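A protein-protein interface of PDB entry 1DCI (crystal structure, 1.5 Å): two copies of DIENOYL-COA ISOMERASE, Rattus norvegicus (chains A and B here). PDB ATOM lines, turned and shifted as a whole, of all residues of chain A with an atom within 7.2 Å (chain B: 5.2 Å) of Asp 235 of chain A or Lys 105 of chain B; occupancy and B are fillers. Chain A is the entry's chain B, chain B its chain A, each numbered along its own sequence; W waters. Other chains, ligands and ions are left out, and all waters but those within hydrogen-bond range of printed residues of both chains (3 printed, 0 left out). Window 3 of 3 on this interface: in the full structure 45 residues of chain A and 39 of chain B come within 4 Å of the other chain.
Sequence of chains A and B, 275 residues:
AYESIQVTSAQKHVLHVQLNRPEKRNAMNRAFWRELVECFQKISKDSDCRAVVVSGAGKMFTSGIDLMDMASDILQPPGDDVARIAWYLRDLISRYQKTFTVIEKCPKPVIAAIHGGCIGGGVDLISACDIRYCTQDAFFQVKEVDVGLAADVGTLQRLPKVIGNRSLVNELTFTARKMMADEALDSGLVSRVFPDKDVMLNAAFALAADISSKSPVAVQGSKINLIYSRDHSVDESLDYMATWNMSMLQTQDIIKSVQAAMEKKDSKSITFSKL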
ATOM      1  N   HIS A 232      10.554 -26.199   4.924  1.00  0.00           N
ATOM      2  CA  HIS A 232      10.334 -25.298   6.044  1.00  0.00           C
ATOM      3  C   HIS A 232      10.955 -25.906   7.292  1.00  0.00           C
ATOM      4  O   HIS A 232      11.292 -27.085   7.301  1.00  0.00           O
ATOM      5  CB  HIS A 232       8.824 -25.064   6.271  1.00  0.00           C
ATOM      6  CG  HIS A 232       8.145 -24.467   5.078  1.00  0.00           C
ATOM      7  ND1 HIS A 232       7.731 -25.223   3.993  1.00  0.00           N
ATOM      8  CD2 HIS A 232       7.863 -23.167   4.773  1.00  0.00           C
ATOM      9  CE1 HIS A 232       7.204 -24.407   3.090  1.00  0.00           C
ATOM     10  NE2 HIS A 232       7.270 -23.174   3.535  1.00  0.00           N
ATOM     11  N   SER A 233      11.103 -25.093   8.328  1.00  0.00           N
ATOM     12  CA  SER A 233      11.699 -25.621   9.568  1.00  0.00           C
ATOM     13  C   SER A 233      10.768 -26.657  10.182  1.00  0.00           C
ATOM     14  O   SER A 233       9.558 -26.670   9.888  1.00  0.00           O
ATOM     15  CB  SER A 233      11.908 -24.466  10.547  1.00  0.00           C
ATOM     16  OG  SER A 233      10.676 -24.046  11.079  1.00  0.00           O
ATOM     17  N   VAL A 234      11.258 -27.499  11.076  1.00  0.00           N
ATOM     18  CA  VAL A 234      10.372 -28.458  11.747  1.00  0.00           C
ATOM     19  C   VAL A 234       9.266 -27.722  12.469  1.00  0.00           C
ATOM     20  O   VAL A 234       8.088 -28.123  12.344  1.00  0.00           O
ATOM     21  CB  VAL A 234      11.156 -29.383  12.693  1.00  0.00           C
ATOM     22  CG1 VAL A 234      10.250 -30.183  13.623  1.00  0.00           C
ATOM     23  CG2 VAL A 234      12.035 -30.324  11.873  1.00  0.00           C
ATOM     24  N   ASP A 235       9.513 -26.667  13.223  1.00  0.00           N
ATOM     25  CA  ASP A 235       8.443 -25.976  13.947  1.00  0.00           C
ATOM     26  C   ASP A 235       7.445 -25.338  12.990  1.00  0.00           C
ATOM     27  O   ASP A 235       6.229 -25.423  13.243  1.00  0.00           O
ATOM     28  CB  ASP A 235       8.988 -24.924  14.914  1.00  0.00           C
ATOM     29  CG  ASP A 235       9.753 -25.515  16.078  1.00  0.00           C
ATOM     30  OD1 ASP A 235       9.534 -26.668  16.477  1.00  0.00           O
ATOM     31  OD2 ASP A 235      10.614 -24.773  16.630  1.00  0.00           O
ATOM     32  N   GLU A 236       7.887 -24.748  11.868  1.00  0.00           N
ATOM     33  CA  GLU A 236       6.918 -24.182  10.928  1.00  0.00           C
ATOM     34  C   GLU A 236       6.070 -25.317  10.339  1.00  0.00           C
ATOM     35  O   GLU A 236       4.857 -25.159  10.099  1.00  0.00           O
ATOM     36  CB  GLU A 236       7.594 -23.486   9.744  1.00  0.00           C
ATOM     37  CG  GLU A 236       8.364 -22.238  10.042  1.00  0.00           C
ATOM     38  CD  GLU A 236       9.348 -21.741   9.004  1.00  0.00           C
ATOM     39  OE1 GLU A 236       9.938 -22.460   8.163  1.00  0.00           O
ATOM     40  OE2 GLU A 236       9.622 -20.515   9.066  1.00  0.00           O
ATOM     41  N   SER A 237       6.686 -26.444  10.057  1.00  0.00           N
ATOM     42  CA  SER A 237       6.037 -27.602   9.455  1.00  0.00           C
ATOM     43  C   SER A 237       5.059 -28.280  10.401  1.00  0.00           C
ATOM     44  O   SER A 237       3.980 -28.712   9.951  1.00  0.00           O
ATOM     45  CB  SER A 237       7.077 -28.594   8.948  1.00  0.00           C
ATOM     46  OG  SER A 237       7.919 -27.933   7.999  1.00  0.00           O
ATOM     47  N   LEU A 238       5.383 -28.303  11.693  1.00  0.00           N
ATOM     48  CA  LEU A 238       4.421 -28.815  12.678  1.00  0.00           C
ATOM     49  C   LEU A 238       3.226 -27.885  12.789  1.00  0.00           C
ATOM     50  O   LEU A 238       2.096 -28.392  12.881  1.00  0.00           O
ATOM     51  CB  LEU A 238       5.099 -28.956  14.052  1.00  0.00           C
ATOM     52  CG  LEU A 238       6.089 -30.104  14.163  1.00  0.00           C
ATOM     53  CD1 LEU A 238       6.981 -29.948  15.407  1.00  0.00           C
ATOM     54  CD2 LEU A 238       5.446 -31.480  14.169  1.00  0.00           C
ATOM     55  N   ASP A 239       3.427 -26.581  12.726  1.00  0.00           N
ATOM     56  CA  ASP A 239       2.313 -25.634  12.799  1.00  0.00           C
ATOM     57  C   ASP A 239       1.409 -25.807  11.582  1.00  0.00           C
ATOM     58  O   ASP A 239       0.164 -25.836  11.703  1.00  0.00           O
ATOM     59  CB  ASP A 239       2.878 -24.234  12.952  1.00  0.00           C
ATOM     60  CG  ASP A 239       1.832 -23.149  12.891  1.00  0.00           C
ATOM     61  OD1 ASP A 239       1.443 -22.759  11.778  1.00  0.00           O
ATOM     62  OD2 ASP A 239       1.363 -22.713  13.964  1.00  0.00           O
ATOM     63  N   TYR A 240       2.017 -25.959  10.411  1.00  0.00           N
ATOM     64  CA  TYR A 240       1.228 -26.183   9.185  1.00  0.00           C
ATOM     65  C   TYR A 240       0.466 -27.495   9.298  1.00  0.00           C
ATOM     66  O   TYR A 240      -0.722 -27.509   8.876  1.00  0.00           O
ATOM     67  CB  TYR A 240       2.163 -26.256   7.975  1.00  0.00           C
ATOM     68  CG  TYR A 240       1.433 -26.186   6.641  1.00  0.00           C
ATOM     69  CD1 TYR A 240       1.150 -24.905   6.166  1.00  0.00           C
ATOM     70  CD2 TYR A 240       1.071 -27.301   5.914  1.00  0.00           C
ATOM     71  CE1 TYR A 240       0.501 -24.744   4.952  1.00  0.00           C
ATOM     72  CE2 TYR A 240       0.400 -27.153   4.702  1.00  0.00           C
ATOM     73  CZ  TYR A 240       0.142 -25.883   4.250  1.00  0.00           C
ATOM     74  OH  TYR A 240      -0.487 -25.680   3.027  1.00  0.00           O
ATOM     75  N   MET A 241       1.063 -28.541   9.818  1.00  0.00           N
ATOM     76  CA  MET A 241       0.439 -29.841   9.961  1.00  0.00           C
ATOM     77  C   MET A 241      -0.779 -29.757  10.883  1.00  0.00           C
ATOM     78  O   MET A 241      -1.783 -30.451  10.607  1.00  0.00           O
ATOM     79  CB  MET A 241       1.458 -30.835  10.505  1.00  0.00           C
ATOM     80  CG  MET A 241       0.967 -32.275  10.618  1.00  0.00           C
ATOM     81  SD  MET A 241       0.843 -32.815   8.902  1.00  0.00           S
ATOM     82  CE  MET A 241      -0.418 -34.091   9.017  1.00  0.00           C
ATOM     83  N   SER B  44      14.966 -30.932  30.982  1.00  0.00           N
ATOM     84  CA  SER B  44      15.618 -29.777  30.376  1.00  0.00           C
ATOM     85  C   SER B  44      16.161 -28.798  31.408  1.00  0.00           C
ATOM     86  O   SER B  44      17.167 -28.160  31.115  1.00  0.00           O
ATOM     87  CB  SER B  44      14.684 -29.031  29.408  1.00  0.00           C
ATOM     88  OG  SER B  44      14.288 -29.977  28.420  1.00  0.00           O
ATOM     89  N   THR B 101       8.227 -32.868  20.591  1.00  0.00           N
ATOM     90  CA  THR B 101       9.042 -31.656  20.404  1.00  0.00           C
ATOM     91  C   THR B 101       9.854 -31.352  21.656  1.00  0.00           C
ATOM     92  O   THR B 101      10.992 -30.902  21.524  1.00  0.00           O
ATOM     93  CB  THR B 101       8.157 -30.464  20.035  1.00  0.00           C
ATOM     94  OG1 THR B 101       7.590 -30.824  18.764  1.00  0.00           O
ATOM     95  CG2 THR B 101       8.960 -29.189  19.861  1.00  0.00           C
ATOM     96  N   VAL B 102       9.341 -31.643  22.852  1.00  0.00           N
ATOM     97  CA  VAL B 102      10.142 -31.417  24.063  1.00  0.00           C
ATOM     98  C   VAL B 102      11.406 -32.263  24.040  1.00  0.00           C
ATOM     99  O   VAL B 102      12.349 -31.819  24.738  1.00  0.00           O
ATOM    100  CB  VAL B 102       9.339 -31.752  25.349  1.00  0.00           C
ATOM    101  CG1 VAL B 102       8.269 -30.689  25.561  1.00  0.00           C
ATOM    102  CG2 VAL B 102       8.765 -33.144  25.323  1.00  0.00           C
ATOM    103  N   ILE B 103      11.495 -33.365  23.324  1.00  0.00           N
ATOM    104  CA  ILE B 103      12.707 -34.163  23.268  1.00  0.00           C
ATOM    105  C   ILE B 103      13.767 -33.406  22.467  1.00  0.00           C
ATOM    106  O   ILE B 103      14.949 -33.381  22.852  1.00  0.00           O
ATOM    107  CB  ILE B 103      12.427 -35.545  22.651  1.00  0.00           C
ATOM    108  CG1 ILE B 103      11.404 -36.295  23.540  1.00  0.00           C
ATOM    109  CG2 ILE B 103      13.713 -36.347  22.555  1.00  0.00           C
ATOM    110  CD1 ILE B 103      10.940 -37.593  22.897  1.00  0.00           C
ATOM    111  N   GLU B 104      13.311 -32.783  21.356  1.00  0.00           N
ATOM    112  CA  GLU B 104      14.249 -31.987  20.548  1.00  0.00           C
ATOM    113  C   GLU B 104      14.665 -30.710  21.259  1.00  0.00           C
ATOM    114  O   GLU B 104      15.838 -30.318  21.154  1.00  0.00           O
ATOM    115  CB  GLU B 104      13.575 -31.698  19.178  1.00  0.00           C
ATOM    116  CG  GLU B 104      14.380 -30.707  18.344  1.00  0.00           C
ATOM    117  CD  GLU B 104      13.812 -30.545  16.920  1.00  0.00           C
ATOM    118  OE1 GLU B 104      13.705 -31.577  16.272  1.00  0.00           O
ATOM    119  OE2 GLU B 104      13.558 -29.372  16.602  1.00  0.00           O
ATOM    120  N   LYS B 105      13.791 -30.039  22.005  1.00  0.00           N
ATOM    121  CA  LYS B 105      14.071 -28.791  22.683  1.00  0.00           C
ATOM    122  C   LYS B 105      14.830 -29.015  23.986  1.00  0.00           C
ATOM    123  O   LYS B 105      15.283 -28.061  24.587  1.00  0.00           O
ATOM    124  CB  LYS B 105      12.769 -27.988  22.878  1.00  0.00           C
ATOM    125  CG  LYS B 105      12.129 -27.794  21.502  1.00  0.00           C
ATOM    126  CD  LYS B 105      11.534 -26.446  21.211  1.00  0.00           C
ATOM    127  CE  LYS B 105      11.055 -26.378  19.764  1.00  0.00           C
ATOM    128  NZ  LYS B 105      11.872 -25.449  18.932  1.00  0.00           N
ATOM    129  N   CYS B 106      14.953 -30.256  24.413  1.00  0.00           N
ATOM    130  CA  CYS B 106      15.774 -30.610  25.579  1.00  0.00           C
ATOM    131  C   CYS B 106      17.225 -30.544  25.103  1.00  0.00           C
ATOM    132  O   CYS B 106      17.570 -31.254  24.171  1.00  0.00           O
ATOM    133  CB  CYS B 106      15.417 -32.026  26.044  1.00  0.00           C
ATOM    134  SG  CYS B 106      16.555 -32.885  27.199  1.00  0.00           S
ATOM    135  N   PRO B 107      18.040 -29.729  25.748  1.00  0.00           N
ATOM    136  CA  PRO B 107      19.421 -29.543  25.303  1.00  0.00           C
ATOM    137  C   PRO B 107      20.308 -30.750  25.497  1.00  0.00           C
ATOM    138  O   PRO B 107      21.373 -30.898  24.878  1.00  0.00           O
ATOM    139  CB  PRO B 107      19.870 -28.302  26.083  1.00  0.00           C
ATOM    140  CG  PRO B 107      19.019 -28.309  27.307  1.00  0.00           C
ATOM    141  CD  PRO B 107      17.672 -28.829  26.861  1.00  0.00           C
ATOM    142  N   ARG B 158      10.190 -34.765  10.780  1.00  0.00           N
ATOM    143  CA  ARG B 158      11.550 -35.122  11.182  1.00  0.00           C
ATOM    144  C   ARG B 158      12.155 -36.348  10.541  1.00  0.00           C
ATOM    145  O   ARG B 158      13.382 -36.378  10.311  1.00  0.00           O
ATOM    146  CB  ARG B 158      11.611 -35.295  12.712  1.00  0.00           C
ATOM    147  CG  ARG B 158      11.272 -34.070  13.521  1.00  0.00           C
ATOM    148  CD  ARG B 158      11.696 -34.215  14.997  1.00  0.00           C
ATOM    149  NE  ARG B 158      11.272 -33.026  15.750  1.00  0.00           N
ATOM    150  CZ  ARG B 158      10.083 -32.830  16.327  1.00  0.00           C
ATOM    151  NH1 ARG B 158       9.153 -33.790  16.260  1.00  0.00           N
ATOM    152  NH2 ARG B 158       9.815 -31.681  16.931  1.00  0.00           N
ATOM    153  N   ASP B 231      17.569 -26.232  10.281  1.00  0.00           N
ATOM    154  CA  ASP B 231      16.396 -25.490   9.803  1.00  0.00           C
ATOM    155  C   ASP B 231      16.677 -24.140   9.192  1.00  0.00           C
ATOM    156  O   ASP B 231      15.726 -23.414   8.855  1.00  0.00           O
ATOM    157  CB  ASP B 231      15.438 -25.326  10.990  1.00  0.00           C
ATOM    158  CG  ASP B 231      14.750 -26.585  11.504  1.00  0.00           C
ATOM    159  OD1 ASP B 231      14.630 -27.552  10.760  1.00  0.00           O
ATOM    160  OD2 ASP B 231      14.460 -26.577  12.723  1.00  0.00           O
HETATM  161  O   HOH W   1      12.283 -25.953  14.141  1.00  0.00           O
HETATM  162  O   HOH W   2      10.892 -29.024  16.954  1.00  0.00           O
HETATM  163  O   HOH W   3      13.953 -24.652   6.629  1.00  0.00           O
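The backbone NH (N) of Val 234 of chain A lies within hydrogen-bond range of the side-chain carboxylate (OD1) of Asp 231 of chain B (3.4 Å). The side-chain amino group (NZ) of Lys 105 of chain B lies within salt-bridge range of the side-chain carboxylate (OD2) of Asp 235 of chain A, at 2.7 Å.
The side-chain hydroxyl of Ser 237 of chain A is in hydrogen-bond range of the backbone carbonyl oxygen of Ser 233 of chain A, 2.8 Å away. NH2 of Arg 158 of chain B lies within hydrogen-bond range of OG1 of Thr 101 of chain B (3.0 Å). The guanidinium group (NE) of Arg 158 of chain B lies within salt-bridge range of the side-chain carboxylate (OE1) of Glu 104 of chain B. The backbone NH of Ser 233 of chain A is in hydrogen-bond range of the side-chain carboxylate of Glu 236 of chain A, at 2.9 Å.
Ser 233 of chain A touches Asp 231 of chain B. Val 234 of chain A touches Arg 158 of chain B (CG1 to NH2, 3.7 Å). CD1 of Leu 238 of chain A touches OG1 of Thr 101 of chain B, at 3.5 Å. NH2 of Arg 158 of chain B touches CD1 of Leu 238 of chain A, at 3.7 Å.
Printed residues of chain B within 4 Å of Val 234 of chain A: Arg 158 (3.7 Å) and Asp 231 (3.4 Å). Of the printed residues of chain B, Leu 238 of chain A touches Thr 101 (3.5 Å) and Arg 158 (3.7 Å). Ser 44 of chain B touches none of the printed residues of chain A. Of chain A, only Asp 235 comes within 4 Å of Lys 105 of chain B. Of the printed residues of chain A, Asp 231 of chain B touches Ser 233 and Val 234. The nearest residue of chain B that does not touch Asp 235 of chain A is Thr 101 of chain B (4.3 Å). The nearest residue of chain A that does not touch Lys 105 of chain B is Leu 238 of chain A (7.0 Å).
Hydrophobic or aromatic side chains of chain A within 4 Å of the printed part of chain B: Val 234 and Leu 238. Of the 10 printed residues of chain B, 4 touch a printed residue of chain A. Among the printed residues, 6 pairs touch across the chains. Among the printed residues, Asp or Glu carboxylates within 4 Å of a Lys or Arg side-chain nitrogen of the other chain: Asp 235 of chain A with Lys 105 of chain B.
No position is printed for both chains. Of the 6 pairs that touch across the chains among the printed residues, none has its exchanged pair printed and touching as well.
Water W1 lies within hydrogen-bond range of the side-chain carboxylate of Asp 231 of chain B and the backbone NH of Asp 235 of chain A. Water W2 lies within hydrogen-bond range of OE2 of Glu 104 of chain B (2.7 Å), OD1 of Asp 235 of chain A (2.8 Å) and NH2 of Arg 158 of chain B (2.9 Å). Water W3 bridges the backbone carbonyl oxygen of Asp 231 of chain B and the backbone NH of Ser 233 of chain A.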
